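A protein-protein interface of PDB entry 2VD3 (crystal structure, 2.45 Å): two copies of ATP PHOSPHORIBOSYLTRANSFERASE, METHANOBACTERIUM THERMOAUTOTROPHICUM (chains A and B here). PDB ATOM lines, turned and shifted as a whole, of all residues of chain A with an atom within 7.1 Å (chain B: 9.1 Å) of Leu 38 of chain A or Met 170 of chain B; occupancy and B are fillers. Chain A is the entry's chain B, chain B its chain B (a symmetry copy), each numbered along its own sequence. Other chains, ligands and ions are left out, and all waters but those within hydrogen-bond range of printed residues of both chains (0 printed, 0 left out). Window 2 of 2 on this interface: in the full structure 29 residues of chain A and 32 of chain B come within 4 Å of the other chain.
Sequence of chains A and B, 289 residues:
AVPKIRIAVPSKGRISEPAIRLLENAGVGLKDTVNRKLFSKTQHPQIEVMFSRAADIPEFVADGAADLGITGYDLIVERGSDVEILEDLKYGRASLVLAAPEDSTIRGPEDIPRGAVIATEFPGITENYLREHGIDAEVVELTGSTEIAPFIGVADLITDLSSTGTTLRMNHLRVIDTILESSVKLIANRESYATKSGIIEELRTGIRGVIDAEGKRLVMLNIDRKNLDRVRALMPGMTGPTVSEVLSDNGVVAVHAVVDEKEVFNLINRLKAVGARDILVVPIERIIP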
ATOM      1  N   ARG A   6      29.802 -11.386  -0.630  1.00  0.00           N
ATOM      2  CA  ARG A   6      29.272 -10.041  -0.504  1.00  0.00           C
ATOM      3  C   ARG A   6      30.006  -9.119  -1.463  1.00  0.00           C
ATOM      4  O   ARG A   6      31.239  -9.096  -1.501  1.00  0.00           O
ATOM      5  CB  ARG A   6      29.403  -9.539   0.932  1.00  0.00           C
ATOM      6  CG  ARG A   6      28.696  -8.218   1.183  1.00  0.00           C
ATOM      7  CD  ARG A   6      28.913  -7.734   2.599  1.00  0.00           C
ATOM      8  NE  ARG A   6      28.272  -8.613   3.567  1.00  0.00           N
ATOM      9  CZ  ARG A   6      28.575  -8.652   4.859  1.00  0.00           C
ATOM     10  NH1 ARG A   6      27.929  -9.485   5.661  1.00  0.00           N
ATOM     11  NH2 ARG A   6      29.522  -7.859   5.346  1.00  0.00           N
ATOM     12  N   VAL A   9      28.725  -2.316  -3.438  1.00  0.00           N
ATOM     13  CA  VAL A   9      28.243  -1.540  -4.571  1.00  0.00           C
ATOM     14  C   VAL A   9      27.966  -0.113  -4.098  1.00  0.00           C
ATOM     15  O   VAL A   9      27.400   0.074  -3.019  1.00  0.00           O
ATOM     16  CB  VAL A   9      26.947  -2.177  -5.166  1.00  0.00           C
ATOM     17  CG1 VAL A   9      26.209  -1.219  -6.090  1.00  0.00           C
ATOM     18  CG2 VAL A   9      27.281  -3.450  -5.901  1.00  0.00           C
ATOM     19  N   THR A  33      14.457  -5.837  -2.834  1.00  0.00           N
ATOM     20  CA  THR A  33      15.142  -4.829  -2.026  1.00  0.00           C
ATOM     21  C   THR A  33      14.148  -3.936  -1.271  1.00  0.00           C
ATOM     22  O   THR A  33      13.309  -3.263  -1.880  1.00  0.00           O
ATOM     23  CB  THR A  33      16.125  -3.966  -2.873  1.00  0.00           C
ATOM     24  OG1 THR A  33      16.799  -4.794  -3.833  1.00  0.00           O
ATOM     25  CG2 THR A  33      17.159  -3.294  -1.979  1.00  0.00           C
ATOM     26  N   VAL A  34      14.256  -3.957   0.058  1.00  0.00           N
ATOM     27  CA  VAL A  34      13.369  -3.212   0.956  1.00  0.00           C
ATOM     28  C   VAL A  34      14.035  -1.902   1.395  1.00  0.00           C
ATOM     29  O   VAL A  34      14.289  -1.010   0.580  1.00  0.00           O
ATOM     30  CB  VAL A  34      13.003  -4.047   2.218  1.00  0.00           C
ATOM     31  CG1 VAL A  34      11.758  -3.488   2.897  1.00  0.00           C
ATOM     32  CG2 VAL A  34      12.785  -5.507   1.858  1.00  0.00           C
ATOM     33  N   ARG A  36      19.722   1.732  -2.290  1.00  0.00           N
ATOM     34  CA  ARG A  36      18.376   1.334  -1.891  1.00  0.00           C
ATOM     35  C   ARG A  36      18.295   1.068  -0.386  1.00  0.00           C
ATOM     36  O   ARG A  36      17.703   1.864   0.352  1.00  0.00           O
ATOM     37  CB  ARG A  36      17.913   0.118  -2.690  1.00  0.00           C
ATOM     38  N   LYS A  37      18.878  -0.045   0.066  1.00  0.00           N
ATOM     39  CA  LYS A  37      18.994  -0.336   1.501  1.00  0.00           C
ATOM     40  C   LYS A  37      20.469  -0.325   1.899  1.00  0.00           C
ATOM     41  O   LYS A  37      21.242   0.479   1.361  1.00  0.00           O
ATOM     42  CB  LYS A  37      18.333  -1.670   1.858  1.00  0.00           C
ATOM     43  CG  LYS A  37      17.807  -1.708   3.294  1.00  0.00           C
ATOM     44  CD  LYS A  37      17.363  -3.100   3.713  1.00  0.00           C
ATOM     45  CE  LYS A  37      16.687  -3.006   5.089  1.00  0.00           C
ATOM     46  NZ  LYS A  37      16.370  -4.372   5.653  1.00  0.00           N
ATOM     47  N   LEU A  38      20.855  -1.190   2.842  1.00  0.00           N
ATOM     48  CA  LEU A  38      22.271  -1.399   3.176  1.00  0.00           C
ATOM     49  C   LEU A  38      22.744  -2.765   2.671  1.00  0.00           C
ATOM     50  O   LEU A  38      23.839  -2.882   2.113  1.00  0.00           O
ATOM     51  CB  LEU A  38      22.525  -1.229   4.684  1.00  0.00           C
ATOM     52  CG  LEU A  38      23.928  -1.420   5.291  1.00  0.00           C
ATOM     53  CD1 LEU A  38      25.031  -0.607   4.591  1.00  0.00           C
ATOM     54  CD2 LEU A  38      23.901  -1.093   6.783  1.00  0.00           C
ATOM     55  N   PHE A  39      21.905  -3.784   2.865  1.00  0.00           N
ATOM     56  CA  PHE A  39      22.133  -5.117   2.304  1.00  0.00           C
ATOM     57  C   PHE A  39      20.945  -5.563   1.467  1.00  0.00           C
ATOM     58  O   PHE A  39      19.798  -5.462   1.906  1.00  0.00           O
ATOM     59  CB  PHE A  39      22.377  -6.150   3.402  1.00  0.00           C
ATOM     60  CG  PHE A  39      23.614  -5.905   4.202  1.00  0.00           C
ATOM     61  CD1 PHE A  39      23.542  -5.259   5.434  1.00  0.00           C
ATOM     62  CD2 PHE A  39      24.854  -6.324   3.730  1.00  0.00           C
ATOM     63  CE1 PHE A  39      24.693  -5.032   6.185  1.00  0.00           C
ATOM     64  CE2 PHE A  39      26.006  -6.101   4.471  1.00  0.00           C
ATOM     65  CZ  PHE A  39      25.928  -5.456   5.700  1.00  0.00           C
ATOM     66  N   SER A  40      21.226  -6.060   0.267  1.00  0.00           N
ATOM     67  CA  SER A  40      20.192  -6.585  -0.609  1.00  0.00           C
ATOM     68  C   SER A  40      20.504  -8.003  -1.051  1.00  0.00           C
ATOM     69  O   SER A  40      21.664  -8.358  -1.244  1.00  0.00           O
ATOM     70  CB  SER A  40      20.018  -5.694  -1.841  1.00  0.00           C
ATOM     71  OG  SER A  40      18.917  -6.128  -2.630  1.00  0.00           O
ATOM     72  N   GLU A  48      25.104 -11.549  -2.236  1.00  0.00           N
ATOM     73  CA  GLU A  48      24.435 -10.439  -1.555  1.00  0.00           C
ATOM     74  C   GLU A  48      25.175  -9.129  -1.838  1.00  0.00           C
ATOM     75  O   GLU A  48      26.394  -9.111  -1.952  1.00  0.00           O
ATOM     76  CB  GLU A  48      24.343 -10.742  -0.050  1.00  0.00           C
ATOM     77  CG  GLU A  48      24.385  -9.556   0.910  1.00  0.00           C
ATOM     78  CD  GLU A  48      24.819  -9.973   2.320  1.00  0.00           C
ATOM     79  OE1 GLU A  48      25.954  -9.634   2.728  1.00  0.00           O
ATOM     80  OE2 GLU A  48      24.034 -10.658   3.010  1.00  0.00           O
ATOM     81  N   VAL A  49      24.418  -8.045  -1.973  1.00  0.00           N
ATOM     82  CA  VAL A  49      24.982  -6.717  -2.220  1.00  0.00           C
ATOM     83  C   VAL A  49      25.022  -5.928  -0.916  1.00  0.00           C
ATOM     84  O   VAL A  49      24.033  -5.883  -0.172  1.00  0.00           O
ATOM     85  CB  VAL A  49      24.139  -5.917  -3.271  1.00  0.00           C
ATOM     86  CG1 VAL A  49      24.589  -4.468  -3.354  1.00  0.00           C
ATOM     87  CG2 VAL A  49      24.197  -6.575  -4.653  1.00  0.00           C
ATOM     88  N   MET A  50      26.173  -5.320  -0.638  1.00  0.00           N
ATOM     89  CA  MET A  50      26.262  -4.299   0.400  1.00  0.00           C
ATOM     90  C   MET A  50      26.411  -2.958  -0.285  1.00  0.00           C
ATOM     91  O   MET A  50      27.386  -2.731  -0.987  1.00  0.00           O
ATOM     92  CB  MET A  50      27.451  -4.552   1.333  1.00  0.00           C
ATOM     93  CG  MET A  50      27.619  -3.491   2.415  1.00  0.00           C
ATOM     94  SD  MET A  50      28.896  -3.846   3.639  1.00  0.00           S
ATOM     95  CE  MET A  50      30.386  -3.582   2.688  1.00  0.00           C
ATOM     96  N   PHE A  51      25.441  -2.074  -0.093  1.00  0.00           N
ATOM     97  CA  PHE A  51      25.559  -0.698  -0.583  1.00  0.00           C
ATOM     98  C   PHE A  51      26.534   0.098   0.270  1.00  0.00           C
ATOM     99  O   PHE A  51      26.421   0.133   1.496  1.00  0.00           O
ATOM    100  CB  PHE A  51      24.196  -0.005  -0.643  1.00  0.00           C
ATOM    101  CG  PHE A  51      23.236  -0.667  -1.577  1.00  0.00           C
ATOM    102  CD1 PHE A  51      22.240  -1.505  -1.087  1.00  0.00           C
ATOM    103  CD2 PHE A  51      23.339  -0.470  -2.957  1.00  0.00           C
ATOM    104  CE1 PHE A  51      21.342  -2.130  -1.956  1.00  0.00           C
ATOM    105  CE2 PHE A  51      22.454  -1.085  -3.836  1.00  0.00           C
ATOM    106  CZ  PHE A  51      21.450  -1.922  -3.333  1.00  0.00           C
ATOM    107  N   SER A  52      27.502   0.725  -0.390  1.00  0.00           N
ATOM    108  CA  SER A  52      28.578   1.422   0.295  1.00  0.00           C
ATOM    109  C   SER A  52      28.964   2.677  -0.460  1.00  0.00           C
ATOM    110  O   SER A  52      28.732   2.785  -1.663  1.00  0.00           O
ATOM    111  CB  SER A  52      29.804   0.518   0.410  1.00  0.00           C
ATOM    112  OG  SER A  52      29.425  -0.808   0.742  1.00  0.00           O
ATOM    113  N   GLU B 102      17.126  -8.482  21.424  1.00  0.00           N
ATOM    114  CA  GLU B 102      18.017  -9.648  21.535  1.00  0.00           C
ATOM    115  C   GLU B 102      18.266 -10.094  22.987  1.00  0.00           C
ATOM    116  O   GLU B 102      18.407 -11.289  23.255  1.00  0.00           O
ATOM    117  CB  GLU B 102      19.327  -9.457  20.741  1.00  0.00           C
ATOM    118  CG  GLU B 102      20.390  -8.551  21.368  1.00  0.00           C
ATOM    119  CD  GLU B 102      21.760  -8.650  20.667  1.00  0.00           C
ATOM    120  OE1 GLU B 102      21.824  -8.627  19.417  1.00  0.00           O
ATOM    121  OE2 GLU B 102      22.786  -8.737  21.372  1.00  0.00           O
ATOM    122  N   GLU B 147      11.357  -0.389  14.775  1.00  0.00           N
ATOM    123  CA  GLU B 147      12.668  -0.862  15.281  1.00  0.00           C
ATOM    124  C   GLU B 147      13.134  -0.126  16.529  1.00  0.00           C
ATOM    125  O   GLU B 147      13.899  -0.658  17.321  1.00  0.00           O
ATOM    126  CB  GLU B 147      13.783  -0.712  14.226  1.00  0.00           C
ATOM    127  CG  GLU B 147      13.368  -0.884  12.790  1.00  0.00           C
ATOM    128  CD  GLU B 147      13.079   0.434  12.100  1.00  0.00           C
ATOM    129  OE1 GLU B 147      13.930   1.348  12.170  1.00  0.00           O
ATOM    130  OE2 GLU B 147      12.004   0.547  11.471  1.00  0.00           O
ATOM    131  N   THR B 164      15.697  -9.376   4.355  1.00  0.00           N
ATOM    132  CA  THR B 164      16.946  -9.699   5.045  1.00  0.00           C
ATOM    133  C   THR B 164      16.758  -9.285   6.502  1.00  0.00           C
ATOM    134  O   THR B 164      16.214  -8.203   6.785  1.00  0.00           O
ATOM    135  CB  THR B 164      18.179  -8.971   4.429  1.00  0.00           C
ATOM    136  OG1 THR B 164      18.126  -7.572   4.728  1.00  0.00           O
ATOM    137  CG2 THR B 164      18.237  -9.153   2.912  1.00  0.00           C
ATOM    138  N   GLY B 165      17.188 -10.137   7.428  1.00  0.00           N
ATOM    139  CA  GLY B 165      17.044  -9.836   8.853  1.00  0.00           C
ATOM    140  C   GLY B 165      18.058  -8.828   9.371  1.00  0.00           C
ATOM    141  O   GLY B 165      18.325  -8.772  10.575  1.00  0.00           O
ATOM    142  N   THR B 166      18.602  -8.013   8.467  1.00  0.00           N
ATOM    143  CA  THR B 166      19.759  -7.161   8.782  1.00  0.00           C
ATOM    144  C   THR B 166      19.432  -5.875   9.556  1.00  0.00           C
ATOM    145  O   THR B 166      20.192  -5.487  10.448  1.00  0.00           O
ATOM    146  CB  THR B 166      20.628  -6.867   7.526  1.00  0.00           C
ATOM    147  OG1 THR B 166      19.812  -6.337   6.473  1.00  0.00           O
ATOM    148  CG2 THR B 166      21.311  -8.155   7.042  1.00  0.00           C
ATOM    149  N   THR B 167      18.314  -5.225   9.226  1.00  0.00           N
ATOM    150  CA  THR B 167      17.833  -4.074  10.001  1.00  0.00           C
ATOM    151  C   THR B 167      17.578  -4.494  11.453  1.00  0.00           C
ATOM    152  O   THR B 167      17.962  -3.791  12.396  1.00  0.00           O
ATOM    153  CB  THR B 167      16.554  -3.457   9.384  1.00  0.00           C
ATOM    154  OG1 THR B 167      16.861  -2.922   8.091  1.00  0.00           O
ATOM    155  CG2 THR B 167      15.998  -2.331  10.258  1.00  0.00           C
ATOM    156  N   LEU B 168      16.939  -5.652  11.606  1.00  0.00           N
ATOM    157  CA  LEU B 168      16.696  -6.268  12.906  1.00  0.00           C
ATOM    158  C   LEU B 168      18.003  -6.583  13.646  1.00  0.00           C
ATOM    159  O   LEU B 168      18.128  -6.305  14.841  1.00  0.00           O
ATOM    160  CB  LEU B 168      15.843  -7.535  12.731  1.00  0.00           C
ATOM    161  CG  LEU B 168      14.399  -7.314  12.266  1.00  0.00           C
ATOM    162  CD1 LEU B 168      13.883  -8.475  11.429  1.00  0.00           C
ATOM    163  CD2 LEU B 168      13.481  -7.058  13.444  1.00  0.00           C
ATOM    164  N   ARG B 169      18.971  -7.142  12.923  1.00  0.00           N
ATOM    165  CA  ARG B 169      20.279  -7.460  13.498  1.00  0.00           C
ATOM    166  C   ARG B 169      21.058  -6.225  13.947  1.00  0.00           C
ATOM    167  O   ARG B 169      21.794  -6.282  14.931  1.00  0.00           O
ATOM    168  CB  ARG B 169      21.121  -8.290  12.527  1.00  0.00           C
ATOM    169  CG  ARG B 169      20.670  -9.729  12.425  1.00  0.00           C
ATOM    170  CD  ARG B 169      21.808 -10.655  12.055  1.00  0.00           C
ATOM    171  NE  ARG B 169      21.460 -12.045  12.344  1.00  0.00           N
ATOM    172  CZ  ARG B 169      20.944 -12.897  11.460  1.00  0.00           C
ATOM    173  NH1 ARG B 169      20.661 -14.140  11.833  1.00  0.00           N
ATOM    174  NH2 ARG B 169      20.716 -12.516  10.205  1.00  0.00           N
ATOM    175  N   MET B 170      20.897  -5.117  13.226  1.00  0.00           N
ATOM    176  CA  MET B 170      21.555  -3.865  13.596  1.00  0.00           C
ATOM    177  C   MET B 170      20.953  -3.328  14.879  1.00  0.00           C
ATOM    178  O   MET B 170      21.677  -2.979  15.814  1.00  0.00           O
ATOM    179  CB  MET B 170      21.439  -2.814  12.488  1.00  0.00           C
ATOM    180  CG  MET B 170      22.410  -3.009  11.333  1.00  0.00           C
ATOM    181  SD  MET B 170      22.412  -1.655  10.139  1.00  0.00           S
ATOM    182  CE  MET B 170      20.693  -1.631   9.611  1.00  0.00           C
ATOM    183  N   ASN B 171      19.625  -3.291  14.928  1.00  0.00           N
ATOM    184  CA  ASN B 171      18.916  -2.750  16.083  1.00  0.00           C
ATOM    185  C   ASN B 171      18.744  -3.766  17.204  1.00  0.00           C
ATOM    186  O   ASN B 171      17.872  -3.621  18.061  1.00  0.00           O
ATOM    187  CB  ASN B 171      17.578  -2.160  15.650  1.00  0.00           C
ATOM    188  CG  ASN B 171      17.748  -0.981  14.720  1.00  0.00           C
ATOM    189  OD1 ASN B 171      17.954   0.148  15.166  1.00  0.00           O
ATOM    190  ND2 ASN B 171      17.671  -1.236  13.417  1.00  0.00           N
ATOM    191  N   HIS B 172      19.599  -4.787  17.191  1.00  0.00           N
ATOM    192  CA  HIS B 172      19.633  -5.826  18.216  1.00  0.00           C
ATOM    193  C   HIS B 172      18.250  -6.414  18.510  1.00  0.00           C
ATOM    194  O   HIS B 172      17.775  -6.397  19.649  1.00  0.00           O
ATOM    195  CB  HIS B 172      20.334  -5.307  19.477  1.00  0.00           C
ATOM    196  CG  HIS B 172      21.825  -5.236  19.344  1.00  0.00           C
ATOM    197  ND1 HIS B 172      22.682  -5.758  20.289  1.00  0.00           N
ATOM    198  CD2 HIS B 172      22.608  -4.733  18.362  1.00  0.00           C
ATOM    199  CE1 HIS B 172      23.930  -5.570  19.897  1.00  0.00           C
ATOM    200  NE2 HIS B 172      23.912  -4.950  18.731  1.00  0.00           N
ATOM    201  N   LEU B 173      17.617  -6.926  17.457  1.00  0.00           N
ATOM    202  CA  LEU B 173      16.317  -7.581  17.559  1.00  0.00           C
ATOM    203  C   LEU B 173      16.365  -8.982  16.959  1.00  0.00           C
ATOM    204  O   LEU B 173      17.094  -9.238  15.998  1.00  0.00           O
ATOM    205  CB  LEU B 173      15.222  -6.759  16.876  1.00  0.00           C
ATOM    206  CG  LEU B 173      14.972  -5.317  17.332  1.00  0.00           C
ATOM    207  CD1 LEU B 173      14.189  -4.589  16.275  1.00  0.00           C
ATOM    208  CD2 LEU B 173      14.251  -5.241  18.669  1.00  0.00           C
ATOM    209  N   ARG B 174      15.583  -9.883  17.535  1.00  0.00           N
ATOM    210  CA  ARG B 174      15.592 -11.279  17.132  1.00  0.00           C
ATOM    211  C   ARG B 174      14.192 -11.683  16.693  1.00  0.00           C
ATOM    212  O   ARG B 174      13.212 -11.397  17.383  1.00  0.00           O
ATOM    213  CB  ARG B 174      16.071 -12.149  18.301  1.00  0.00           C
ATOM    214  CG  ARG B 174      16.021 -13.652  18.048  1.00  0.00           C
ATOM    215  CD  ARG B 174      16.403 -14.454  19.287  1.00  0.00           C
ATOM    216  NE  ARG B 174      15.467 -14.245  20.393  1.00  0.00           N
ATOM    217  CZ  ARG B 174      15.780 -13.647  21.539  1.00  0.00           C
ATOM    218  NH1 ARG B 174      17.014 -13.201  21.749  1.00  0.00           N
ATOM    219  NH2 ARG B 174      14.866 -13.502  22.483  1.00  0.00           N
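N of Phe 51 of chain A is in hydrogen-bond range of O of Leu 38 of chain A, 2.8 Å away.
The side-chain hydroxyl of Thr 164 of chain B lies within hydrogen-bond range of the side-chain hydroxyl of Thr 166 of chain B.
ND2 of Asn 171 of chain B lies within hydrogen-bond range of O of Thr 167 of chain B (2.8 Å).
The side-chain amino group (NZ) of Lys 37 of chain A sits at hydrogen-bond distance from the side-chain hydroxyl (OG1) of Thr 167 of chain B, 2.9 Å away.
Hydrophobic or aromatic side chains of chain A that line the printed part of chain B: Leu 38 and Phe 39.
Of the 13 printed residues of chain B, 4 touch a printed residue of chain A.
Hydrophobic or aromatic side chains of chain B within 4 Å of the printed part of chain A: Met 170.
Among the printed residues, pairs that only touch across the chains: Lys 37 of chain A with Thr 164 of chain B, Leu 38 of chain A with Met 170 of chain B, Phe 39 of chain A with Thr 164 of chain B and Phe 39 of chain A with Thr 166 of chain B.
Leu 38 of chain A touches just one residue of chain B: Met 170.
Met 170 of chain B touches one residue of chain A.
Printed residues of chain A within 4 Å of Thr 164 of chain B: Lys 37 and Phe 39.
Of the printed residues of chain B, Lys 37 of chain A touches Thr 164 and Thr 167.
Of the printed residues of chain A, Thr 166 of chain B touches Phe 39.
Val 49 of chain A touches none of the printed residues of chain B.
No position is printed for both chains.
Of the 5 pairs that touch across the chains among the printed residues, none has its exchanged pair printed and touching as well.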
